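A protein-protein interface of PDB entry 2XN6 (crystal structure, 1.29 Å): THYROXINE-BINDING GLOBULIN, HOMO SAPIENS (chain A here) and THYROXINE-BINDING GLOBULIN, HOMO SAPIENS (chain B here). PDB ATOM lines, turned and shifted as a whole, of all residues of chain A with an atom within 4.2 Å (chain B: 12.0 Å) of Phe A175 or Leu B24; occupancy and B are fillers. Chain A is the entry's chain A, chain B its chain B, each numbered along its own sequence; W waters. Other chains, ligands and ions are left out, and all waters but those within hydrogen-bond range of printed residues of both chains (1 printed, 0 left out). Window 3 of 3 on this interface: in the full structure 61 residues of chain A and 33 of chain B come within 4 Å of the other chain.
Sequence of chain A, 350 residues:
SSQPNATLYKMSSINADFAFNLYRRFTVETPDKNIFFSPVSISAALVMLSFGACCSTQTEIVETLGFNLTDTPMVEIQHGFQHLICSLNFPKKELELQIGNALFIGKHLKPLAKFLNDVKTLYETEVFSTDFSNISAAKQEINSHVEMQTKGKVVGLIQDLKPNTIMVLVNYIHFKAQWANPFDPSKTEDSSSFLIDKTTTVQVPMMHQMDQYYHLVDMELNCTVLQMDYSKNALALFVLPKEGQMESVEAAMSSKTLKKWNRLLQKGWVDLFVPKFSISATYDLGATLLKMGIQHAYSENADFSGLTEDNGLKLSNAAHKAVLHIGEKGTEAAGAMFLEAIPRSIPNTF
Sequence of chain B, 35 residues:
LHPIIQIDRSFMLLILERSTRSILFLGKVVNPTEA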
ATOM      1  N   SER A  38      30.064  14.052  -5.189  1.00  0.00           N
ATOM      2  CA  SER A  38      29.717  13.958  -6.594  1.00  0.00           C
ATOM      3  C   SER A  38      30.828  14.522  -7.461  1.00  0.00           C
ATOM      4  O   SER A  38      30.978  15.739  -7.554  1.00  0.00           O
ATOM      5  CB  SER A  38      28.441  14.738  -6.897  1.00  0.00           C
ATOM      6  OG  SER A  38      28.168  14.731  -8.290  1.00  0.00           O
ATOM      7  N   PRO A  39      31.604  13.645  -8.117  1.00  0.00           N
ATOM      8  CA  PRO A  39      32.672  14.164  -8.967  1.00  0.00           C
ATOM      9  C   PRO A  39      32.135  15.000 -10.127  1.00  0.00           C
ATOM     10  O   PRO A  39      32.749  16.000 -10.478  1.00  0.00           O
ATOM     11  CB  PRO A  39      33.375  12.907  -9.478  1.00  0.00           C
ATOM     12  CG  PRO A  39      32.798  11.756  -8.781  1.00  0.00           C
ATOM     13  CD  PRO A  39      31.604  12.172  -8.028  1.00  0.00           C
ATOM     14  N   VAL A  40      31.005  14.598 -10.705  1.00  0.00           N
ATOM     15  CA  VAL A  40      30.444  15.334 -11.840  1.00  0.00           C
ATOM     16  C   VAL A  40      30.038  16.742 -11.420  1.00  0.00           C
ATOM     17  O   VAL A  40      30.212  17.683 -12.188  1.00  0.00           O
ATOM     18  CB  VAL A  40      29.283  14.577 -12.538  1.00  0.00           C
ATOM     19  CG1 VAL A  40      28.074  14.429 -11.641  1.00  0.00           C
ATOM     20  CG2 VAL A  40      28.897  15.272 -13.855  1.00  0.00           C
ATOM     21  N   LEU A  88      22.605  14.099 -19.311  1.00  0.00           N
ATOM     22  CA  LEU A  88      22.221  13.711 -17.950  1.00  0.00           C
ATOM     23  C   LEU A  88      20.807  14.189 -17.593  1.00  0.00           C
ATOM     24  O   LEU A  88      20.065  13.482 -16.909  1.00  0.00           O
ATOM     25  CB  LEU A  88      23.241  14.229 -16.930  1.00  0.00           C
ATOM     26  CG  LEU A  88      24.637  13.601 -16.986  1.00  0.00           C
ATOM     27  CD1 LEU A  88      25.560  14.313 -16.006  1.00  0.00           C
ATOM     28  CD2 LEU A  88      24.598  12.097 -16.707  1.00  0.00           C
ATOM     29  N   LEU A  95      13.641   7.287 -13.619  1.00  0.00           N
ATOM     30  CA  LEU A  95      14.863   7.879 -13.065  1.00  0.00           C
ATOM     31  C   LEU A  95      14.658   9.372 -12.856  1.00  0.00           C
ATOM     32  O   LEU A  95      14.281  10.080 -13.787  1.00  0.00           O
ATOM     33  CB  LEU A  95      16.051   7.660 -14.013  1.00  0.00           C
ATOM     34  CG  LEU A  95      17.361   8.385 -13.657  1.00  0.00           C
ATOM     35  CD1 LEU A  95      17.831   7.996 -12.268  1.00  0.00           C
ATOM     36  CD2 LEU A  95      18.446   8.099 -14.686  1.00  0.00           C
ATOM     37  N   GLU A  96      14.894   9.845 -11.634  1.00  0.00           N
ATOM     38  CA  GLU A  96      15.023  11.276 -11.370  1.00  0.00           C
ATOM     39  C   GLU A  96      16.508  11.616 -11.359  1.00  0.00           C
ATOM     40  O   GLU A  96      17.265  11.102 -10.533  1.00  0.00           O
ATOM     41  CB  GLU A  96      14.403  11.654 -10.024  1.00  0.00           C
ATOM     42  CG  GLU A  96      12.882  11.585  -9.979  1.00  0.00           C
ATOM     43  CD  GLU A  96      12.320  11.747  -8.575  1.00  0.00           C
ATOM     44  OE1 GLU A  96      12.812  12.616  -7.823  1.00  0.00           O
ATOM     45  OE2 GLU A  96      11.378  11.001  -8.223  1.00  0.00           O
ATOM     46  N   LEU A  97      16.932  12.442 -12.304  1.00  0.00           N
ATOM     47  CA  LEU A  97      18.305  12.928 -12.335  1.00  0.00           C
ATOM     48  C   LEU A  97      18.305  14.334 -12.892  1.00  0.00           C
ATOM     49  O   LEU A  97      17.950  14.551 -14.055  1.00  0.00           O
ATOM     50  CB  LEU A  97      19.198  12.021 -13.189  1.00  0.00           C
ATOM     51  CG  LEU A  97      20.669  12.423 -13.379  1.00  0.00           C
ATOM     52  CD1 LEU A  97      21.385  12.647 -12.052  1.00  0.00           C
ATOM     53  CD2 LEU A  97      21.388  11.371 -14.207  1.00  0.00           C
ATOM     54  N   HIS A 174      20.784  16.101  -8.193  1.00  0.00           N
ATOM     55  CA  HIS A 174      19.860  15.286  -7.417  1.00  0.00           C
ATOM     56  C   HIS A 174      19.557  14.018  -8.198  1.00  0.00           C
ATOM     57  O   HIS A 174      19.319  14.073  -9.393  1.00  0.00           O
ATOM     58  CB  HIS A 174      18.573  16.045  -7.129  1.00  0.00           C
ATOM     59  CG  HIS A 174      17.539  15.196  -6.474  1.00  0.00           C
ATOM     60  ND1 HIS A 174      16.505  14.616  -7.174  1.00  0.00           N
ATOM     61  CD2 HIS A 174      17.423  14.760  -5.198  1.00  0.00           C
ATOM     62  CE1 HIS A 174      15.776  13.885  -6.350  1.00  0.00           C
ATOM     63  NE2 HIS A 174      16.311  13.954  -5.146  1.00  0.00           N
ATOM     64  N   PHE A 175      19.572  12.888  -7.498  1.00  0.00           N
ATOM     65  CA  PHE A 175      19.420  11.566  -8.096  1.00  0.00           C
ATOM     66  C   PHE A 175      18.477  10.750  -7.216  1.00  0.00           C
ATOM     67  O   PHE A 175      18.657  10.675  -6.007  1.00  0.00           O
ATOM     68  CB  PHE A 175      20.802  10.885  -8.180  1.00  0.00           C
ATOM     69  CG  PHE A 175      20.769   9.428  -8.593  1.00  0.00           C
ATOM     70  CD1 PHE A 175      20.742   9.068  -9.924  1.00  0.00           C
ATOM     71  CD2 PHE A 175      20.824   8.417  -7.645  1.00  0.00           C
ATOM     72  CE1 PHE A 175      20.748   7.733 -10.307  1.00  0.00           C
ATOM     73  CE2 PHE A 175      20.812   7.081  -8.027  1.00  0.00           C
ATOM     74  CZ  PHE A 175      20.776   6.746  -9.357  1.00  0.00           C
ATOM     75  N   LYS A 176      17.457  10.155  -7.818  1.00  0.00           N
ATOM     76  CA  LYS A 176      16.578   9.243  -7.093  1.00  0.00           C
ATOM     77  C   LYS A 176      16.139   8.147  -8.036  1.00  0.00           C
ATOM     78  O   LYS A 176      15.610   8.413  -9.114  1.00  0.00           O
ATOM     79  CB  LYS A 176      15.383   9.984  -6.512  1.00  0.00           C
ATOM     80  CG  LYS A 176      14.567   9.177  -5.519  1.00  0.00           C
ATOM     81  CD  LYS A 176      13.438  10.045  -4.983  1.00  0.00           C
ATOM     82  CE  LYS A 176      12.587   9.353  -3.930  1.00  0.00           C
ATOM     83  NZ  LYS A 176      11.454  10.221  -3.479  1.00  0.00           N
ATOM     84  N   ALA A 177      16.373   6.908  -7.627  1.00  0.00           N
ATOM     85  CA  ALA A 177      16.144   5.770  -8.506  1.00  0.00           C
ATOM     86  C   ALA A 177      15.723   4.573  -7.685  1.00  0.00           C
ATOM     87  O   ALA A 177      16.033   4.489  -6.504  1.00  0.00           O
ATOM     88  CB  ALA A 177      17.398   5.454  -9.308  1.00  0.00           C
ATOM     89  N   TYR A 230      19.873   0.048 -11.202  1.00  0.00           N
ATOM     90  CA  TYR A 230      18.628   0.775 -10.990  1.00  0.00           C
ATOM     91  C   TYR A 230      17.741   0.410 -12.170  1.00  0.00           C
ATOM     92  O   TYR A 230      18.205  -0.216 -13.130  1.00  0.00           O
ATOM     93  CB  TYR A 230      18.880   2.280 -10.858  1.00  0.00           C
ATOM     94  CG  TYR A 230      19.713   2.592  -9.639  1.00  0.00           C
ATOM     95  CD1 TYR A 230      21.041   2.959  -9.760  1.00  0.00           C
ATOM     96  CD2 TYR A 230      19.183   2.493  -8.366  1.00  0.00           C
ATOM     97  CE1 TYR A 230      21.820   3.220  -8.657  1.00  0.00           C
ATOM     98  CE2 TYR A 230      19.956   2.764  -7.241  1.00  0.00           C
ATOM     99  CZ  TYR A 230      21.276   3.130  -7.399  1.00  0.00           C
ATOM    100  OH  TYR A 230      22.078   3.394  -6.307  1.00  0.00           O
ATOM    101  N   ALA A 234      21.056   3.567 -15.017  1.00  0.00           N
ATOM    102  CA  ALA A 234      21.992   3.796 -13.923  1.00  0.00           C
ATOM    103  C   ALA A 234      22.261   2.521 -13.139  1.00  0.00           C
ATOM    104  O   ALA A 234      21.474   1.579 -13.172  1.00  0.00           O
ATOM    105  CB  ALA A 234      21.459   4.887 -13.006  1.00  0.00           C
ATOM    106  N   THR A 331      17.781   4.239  -4.093  1.00  0.00           N
ATOM    107  CA  THR A 331      18.790   5.164  -3.613  1.00  0.00           C
ATOM    108  C   THR A 331      18.347   6.582  -3.905  1.00  0.00           C
ATOM    109  O   THR A 331      17.780   6.855  -4.957  1.00  0.00           O
ATOM    110  CB  THR A 331      20.139   4.933  -4.333  1.00  0.00           C
ATOM    111  OG1 THR A 331      20.626   3.628  -4.037  1.00  0.00           O
ATOM    112  CG2 THR A 331      21.193   5.946  -3.901  1.00  0.00           C
ATOM    113  N   GLU A 332      18.629   7.488  -2.982  1.00  0.00           N
ATOM    114  CA  GLU A 332      18.519   8.913  -3.246  1.00  0.00           C
ATOM    115  C   GLU A 332      19.824   9.561  -2.822  1.00  0.00           C
ATOM    116  O   GLU A 332      20.324   9.294  -1.736  1.00  0.00           O
ATOM    117  CB  GLU A 332      17.343   9.541  -2.500  1.00  0.00           C
ATOM    118  CG  GLU A 332      17.108  10.998  -2.885  1.00  0.00           C
ATOM    119  CD  GLU A 332      15.735  11.524  -2.521  1.00  0.00           C
ATOM    120  OE1 GLU A 332      15.029  10.901  -1.692  1.00  0.00           O
ATOM    121  OE2 GLU A 332      15.362  12.587  -3.065  1.00  0.00           O
ATOM    122  N   ALA A 333      20.381  10.389  -3.699  1.00  0.00           N
ATOM    123  CA  ALA A 333      21.645  11.060  -3.431  1.00  0.00           C
ATOM    124  C   ALA A 333      21.588  12.455  -4.018  1.00  0.00           C
ATOM    125  O   ALA A 333      20.899  12.685  -5.003  1.00  0.00           O
ATOM    126  CB  ALA A 333      22.825  10.267  -4.015  1.00  0.00           C
ATOM    127  N   LEU B  13      31.785   2.740  -2.932  1.00  0.00           N
ATOM    128  CA  LEU B  13      30.531   2.800  -3.656  1.00  0.00           C
ATOM    129  C   LEU B  13      30.654   3.767  -4.814  1.00  0.00           C
ATOM    130  O   LEU B  13      31.177   4.871  -4.638  1.00  0.00           O
ATOM    131  CB  LEU B  13      29.426   3.300  -2.725  1.00  0.00           C
ATOM    132  CG  LEU B  13      28.034   3.537  -3.307  1.00  0.00           C
ATOM    133  CD1 LEU B  13      27.428   2.211  -3.773  1.00  0.00           C
ATOM    134  CD2 LEU B  13      27.103   4.250  -2.320  1.00  0.00           C
ATOM    135  N   LEU B  14      30.154   3.363  -5.977  1.00  0.00           N
ATOM    136  CA  LEU B  14      30.067   4.235  -7.146  1.00  0.00           C
ATOM    137  C   LEU B  14      28.645   4.219  -7.661  1.00  0.00           C
ATOM    138  O   LEU B  14      28.042   3.149  -7.739  1.00  0.00           O
ATOM    139  CB  LEU B  14      30.992   3.738  -8.263  1.00  0.00           C
ATOM    140  CG  LEU B  14      32.491   3.657  -7.977  1.00  0.00           C
ATOM    141  CD1 LEU B  14      32.861   2.364  -7.266  1.00  0.00           C
ATOM    142  CD2 LEU B  14      33.277   3.787  -9.280  1.00  0.00           C
ATOM    143  N   ILE B  15      28.112   5.379  -8.028  1.00  0.00           N
ATOM    144  CA  ILE B  15      26.834   5.458  -8.729  1.00  0.00           C
ATOM    145  C   ILE B  15      27.136   5.995 -10.114  1.00  0.00           C
ATOM    146  O   ILE B  15      27.686   7.088 -10.250  1.00  0.00           O
ATOM    147  CB  ILE B  15      25.829   6.354  -7.993  1.00  0.00           C
ATOM    148  CG1 ILE B  15      25.527   5.751  -6.616  1.00  0.00           C
ATOM    149  CG2 ILE B  15      24.543   6.525  -8.816  1.00  0.00           C
ATOM    150  CD1 ILE B  15      24.643   6.612  -5.751  1.00  0.00           C
ATOM    151  N   LEU B  16      26.806   5.192 -11.123  1.00  0.00           N
ATOM    152  CA  LEU B  16      27.187   5.463 -12.510  1.00  0.00           C
ATOM    153  C   LEU B  16      25.947   5.656 -13.384  1.00  0.00           C
ATOM    154  O   LEU B  16      24.945   4.967 -13.215  1.00  0.00           O
ATOM    155  CB  LEU B  16      28.002   4.289 -13.068  1.00  0.00           C
ATOM    156  CG  LEU B  16      29.165   3.782 -12.201  1.00  0.00           C
ATOM    157  CD1 LEU B  16      29.787   2.513 -12.770  1.00  0.00           C
ATOM    158  CD2 LEU B  16      30.213   4.854 -12.050  1.00  0.00           C
ATOM    159  N   GLU B  17      26.025   6.583 -14.336  1.00  0.00           N
ATOM    160  CA  GLU B  17      24.999   6.747 -15.364  1.00  0.00           C
ATOM    161  C   GLU B  17      25.535   6.100 -16.637  1.00  0.00           C
ATOM    162  O   GLU B  17      26.669   6.338 -17.039  1.00  0.00           O
ATOM    163  CB  GLU B  17      24.683   8.232 -15.564  1.00  0.00           C
ATOM    164  CG  GLU B  17      23.458   8.529 -16.420  1.00  0.00           C
ATOM    165  CD  GLU B  17      23.743   8.467 -17.908  1.00  0.00           C
ATOM    166  OE1 GLU B  17      24.904   8.678 -18.307  1.00  0.00           O
ATOM    167  OE2 GLU B  17      22.809   8.199 -18.685  1.00  0.00           O
ATOM    168  N   ARG B  18      24.711   5.277 -17.274  1.00  0.00           N
ATOM    169  CA  ARG B  18      25.174   4.431 -18.381  1.00  0.00           C
ATOM    170  C   ARG B  18      25.472   5.166 -19.684  1.00  0.00           C
ATOM    171  O   ARG B  18      26.524   4.957 -20.294  1.00  0.00           O
ATOM    172  CB  ARG B  18      24.148   3.339 -18.681  1.00  0.00           C
ATOM    173  CG  ARG B  18      24.255   2.131 -17.791  1.00  0.00           C
ATOM    174  CD  ARG B  18      23.669   0.919 -18.492  1.00  0.00           C
ATOM    175  NE  ARG B  18      23.931  -0.317 -17.765  1.00  0.00           N
ATOM    176  CZ  ARG B  18      23.267  -0.723 -16.684  1.00  0.00           C
ATOM    177  NH1 ARG B  18      22.287   0.013 -16.164  1.00  0.00           N
ATOM    178  NH2 ARG B  18      23.596  -1.873 -16.111  1.00  0.00           N
ATOM    179  N   SER B  19      24.540   6.001 -20.127  1.00  0.00           N
ATOM    180  CA  SER B  19      24.627   6.574 -21.474  1.00  0.00           C
ATOM    181  C   SER B  19      25.829   7.502 -21.662  1.00  0.00           C
ATOM    182  O   SER B  19      26.343   7.633 -22.772  1.00  0.00           O
ATOM    183  CB  SER B  19      23.330   7.298 -21.844  1.00  0.00           C
ATOM    184  OG  SER B  19      23.202   8.524 -21.157  1.00  0.00           O
ATOM    185  N   THR B  20      26.271   8.146 -20.585  1.00  0.00           N
ATOM    186  CA  THR B  20      27.425   9.039 -20.632  1.00  0.00           C
ATOM    187  C   THR B  20      28.663   8.435 -19.967  1.00  0.00           C
ATOM    188  O   THR B  20      29.747   9.019 -20.021  1.00  0.00           O
ATOM    189  CB  THR B  20      27.114  10.363 -19.929  1.00  0.00           C
ATOM    190  OG1 THR B  20      26.940  10.129 -18.526  1.00  0.00           O
ATOM    191  CG2 THR B  20      25.848  10.988 -20.499  1.00  0.00           C
ATOM    192  N   ARG B  21      28.483   7.288 -19.307  1.00  0.00           N
ATOM    193  CA  ARG B  21      29.529   6.640 -18.500  1.00  0.00           C
ATOM    194  C   ARG B  21      30.104   7.566 -17.421  1.00  0.00           C
ATOM    195  O   ARG B  21      31.305   7.568 -17.144  1.00  0.00           O
ATOM    196  CB  ARG B  21      30.638   6.078 -19.399  1.00  0.00           C
ATOM    197  CG  ARG B  21      30.153   4.982 -20.329  1.00  0.00           C
ATOM    198  CD  ARG B  21      31.158   4.678 -21.421  1.00  0.00           C
ATOM    199  NE  ARG B  21      30.800   3.490 -22.197  1.00  0.00           N
ATOM    200  CZ  ARG B  21      29.805   3.421 -23.083  1.00  0.00           C
ATOM    201  NH1 ARG B  21      29.022   4.470 -23.323  1.00  0.00           N
ATOM    202  NH2 ARG B  21      29.582   2.284 -23.737  1.00  0.00           N
ATOM    203  N   SER B  22      29.222   8.334 -16.799  1.00  0.00           N
ATOM    204  CA  SER B  22      29.621   9.302 -15.786  1.00  0.00           C
ATOM    205  C   SER B  22      29.538   8.712 -14.390  1.00  0.00           C
ATOM    206  O   SER B  22      28.579   8.020 -14.063  1.00  0.00           O
ATOM    207  CB  SER B  22      28.709  10.521 -15.828  1.00  0.00           C
ATOM    208  OG  SER B  22      28.878  11.235 -17.028  1.00  0.00           O
ATOM    209  N   ILE B  23      30.540   8.993 -13.566  1.00  0.00           N
ATOM    210  CA  ILE B  23      30.460   8.700 -12.142  1.00  0.00           C
ATOM    211  C   ILE B  23      29.709   9.870 -11.505  1.00  0.00           C
ATOM    212  O   ILE B  23      30.253  10.978 -11.346  1.00  0.00           O
ATOM    213  CB  ILE B  23      31.841   8.549 -11.473  1.00  0.00           C
ATOM    214  CG1 ILE B  23      32.654   7.434 -12.143  1.00  0.00           C
ATOM    215  CG2 ILE B  23      31.655   8.273  -9.988  1.00  0.00           C
ATOM    216  CD1 ILE B  23      34.077   7.315 -11.615  1.00  0.00           C
ATOM    217  N   LEU B  24      28.461   9.623 -11.141  1.00  0.00           N
ATOM    218  CA  LEU B  24      27.625  10.636 -10.497  1.00  0.00           C
ATOM    219  C   LEU B  24      28.019  10.864  -9.043  1.00  0.00           C
ATOM    220  O   LEU B  24      28.035  11.997  -8.571  1.00  0.00           O
ATOM    221  CB  LEU B  24      26.163  10.224 -10.562  1.00  0.00           C
ATOM    222  CG  LEU B  24      25.558   9.974 -11.941  1.00  0.00           C
ATOM    223  CD1 LEU B  24      24.085   9.628 -11.778  1.00  0.00           C
ATOM    224  CD2 LEU B  24      25.740  11.170 -12.867  1.00  0.00           C
ATOM    225  N   PHE B  25      28.303   9.779  -8.326  1.00  0.00           N
ATOM    226  CA  PHE B  25      28.695   9.830  -6.919  1.00  0.00           C
ATOM    227  C   PHE B  25      29.756   8.763  -6.668  1.00  0.00           C
ATOM    228  O   PHE B  25      29.725   7.696  -7.283  1.00  0.00           O
ATOM    229  CB  PHE B  25      27.495   9.581  -6.001  1.00  0.00           C
ATOM    230  CG  PHE B  25      26.406  10.597  -6.155  1.00  0.00           C
ATOM    231  CD1 PHE B  25      26.432  11.781  -5.444  1.00  0.00           C
ATOM    232  CD2 PHE B  25      25.359  10.381  -7.032  1.00  0.00           C
ATOM    233  CE1 PHE B  25      25.429  12.731  -5.605  1.00  0.00           C
ATOM    234  CE2 PHE B  25      24.351  11.340  -7.193  1.00  0.00           C
ATOM    235  CZ  PHE B  25      24.400  12.505  -6.476  1.00  0.00           C
ATOM    236  N   LEU B  26      30.650   9.028  -5.719  1.00  0.00           N
ATOM    237  CA  LEU B  26      31.756   8.151  -5.362  1.00  0.00           C
ATOM    238  C   LEU B  26      31.956   8.291  -3.872  1.00  0.00           C
ATOM    239  O   LEU B  26      31.947   9.392  -3.334  1.00  0.00           O
ATOM    240  CB  LEU B  26      33.020   8.567  -6.115  1.00  0.00           C
ATOM    241  CG  LEU B  26      34.316   7.833  -5.776  1.00  0.00           C
ATOM    242  CD1 LEU B  26      34.211   6.322  -5.985  1.00  0.00           C
ATOM    243  CD2 LEU B  26      35.449   8.394  -6.618  1.00  0.00           C
ATOM    244  N   GLY B  27      32.170   7.176  -3.192  1.00  0.00           N
ATOM    245  CA  GLY B  27      32.443   7.249  -1.779  1.00  0.00           C
ATOM    246  C   GLY B  27      33.026   5.995  -1.182  1.00  0.00           C
ATOM    247  O   GLY B  27      33.219   4.981  -1.860  1.00  0.00           O
ATOM    248  N   LYS B  28      33.311   6.100   0.104  1.00  0.00           N
ATOM    249  CA  LYS B  28      33.722   4.977   0.926  1.00  0.00           C
ATOM    250  C   LYS B  28      32.895   5.034   2.189  1.00  0.00           C
ATOM    251  O   LYS B  28      32.810   6.074   2.847  1.00  0.00           O
ATOM    252  CB  LYS B  28      35.192   5.067   1.284  1.00  0.00           C
ATOM    253  CG  LYS B  28      35.651   3.988   2.271  1.00  0.00           C
ATOM    254  CD  LYS B  28      37.161   3.966   2.460  1.00  0.00           C
ATOM    255  CE  LYS B  28      37.707   5.317   2.917  1.00  0.00           C
ATOM    256  NZ  LYS B  28      39.165   5.273   3.229  1.00  0.00           N
HETATM  257  O   HOH W   1      19.825   0.249 -15.349  1.00  0.00           O
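The backbone carbonyl oxygen of Leu B24 lies within hydrogen-bond range of the side-chain hydroxyl of Ser A38 (2.8 Å). O of Ala A234 is in hydrogen-bond range of NH1 of Arg B18 (3.5 Å).
OE2 of Glu B17 is in hydrogen-bond range of OG of Ser B19 (2.5 Å). OH of Tyr A230 sits at hydrogen-bond distance from OG1 of Thr A331 (2.7 Å). The backbone NH (N) of Glu B17 is in hydrogen-bond range of the backbone carbonyl oxygen (O) of Ser B22 (2.9 Å). O of Phe B25 is in hydrogen-bond range of N of Ile B15, at 2.9 Å. OG1 of Thr B20 lies within hydrogen-bond range of OG of Ser B22 (2.7 Å). O of Ala A177 is in hydrogen-bond range of N of Thr A331 (3.0 Å).
Among the printed residues, pairs that only touch across the chains: Ala A234 with Leu B16, Leu A88 with Thr B20, Pro A39 with Leu B24, Ala A333 with Phe B25, Pro A39 with Ile B23, Phe A175 with Phe B25, Val A40 with Ile B23, Leu A88 with Glu B17, Phe A175 with Ile B15, Ser A38 with Phe B25, Phe A175 with Leu B24, Pro A39 with Phe B25, Val A40 with Leu B24 and Thr A331 with Ile B15.
Phe A175 touches just these residues of chain B: Ile B15, Leu B24 and Phe B25. Of chain B, only Leu B24 (2.8 Å) and Phe B25 (3.8 Å) come within 4 Å of Ser A38. Leu A88 touches just these residues of chain B: Glu B17 and Thr B20. No residue of chain B comes within 4 Å of Leu A95. No residue of chain B comes within 4 Å of Glu A96. No residue of chain B comes within 4 Å of Leu A97. His A174 touches none of the printed residues of chain B. Ala A177 touches none of the printed residues of chain B. Thr A331 touches just one residue of chain B: Ile B15 (3.97 Å). Of the printed residues of chain A, Arg B18 touches Ala A234 (3.5 Å). Printed residues of chain A within 4 Å of Phe B25: Ser A38 (3.8 Å), Pro A39 (3.9 Å), Phe A175 (3.7 Å) and Ala A333 (3.7 Å). Ser B22 touches none of the printed residues of chain A. Ser B19 touches none of the printed residues of chain A. The nearest residue of chain A that does not touch Leu B24 is Leu A97 (4.03 Å).
Of the 16 printed residues of chain A, 8 touch a printed residue of chain B. Hydrophobic or aromatic side chains of chain B that line the printed part of chain A: Ile B15, Ile B23, Leu B24 and Phe B25. Among the printed residues, no Asp or Glu carboxylate lies within 4 Å of a Lys or Arg side-chain nitrogen of the other chain.
Water W1 lies within hydrogen-bond range of NH1 of Arg B18 (2.6 Å), O of Tyr A230 (2.8 Å) and O of Ala A234 (3.0 Å).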
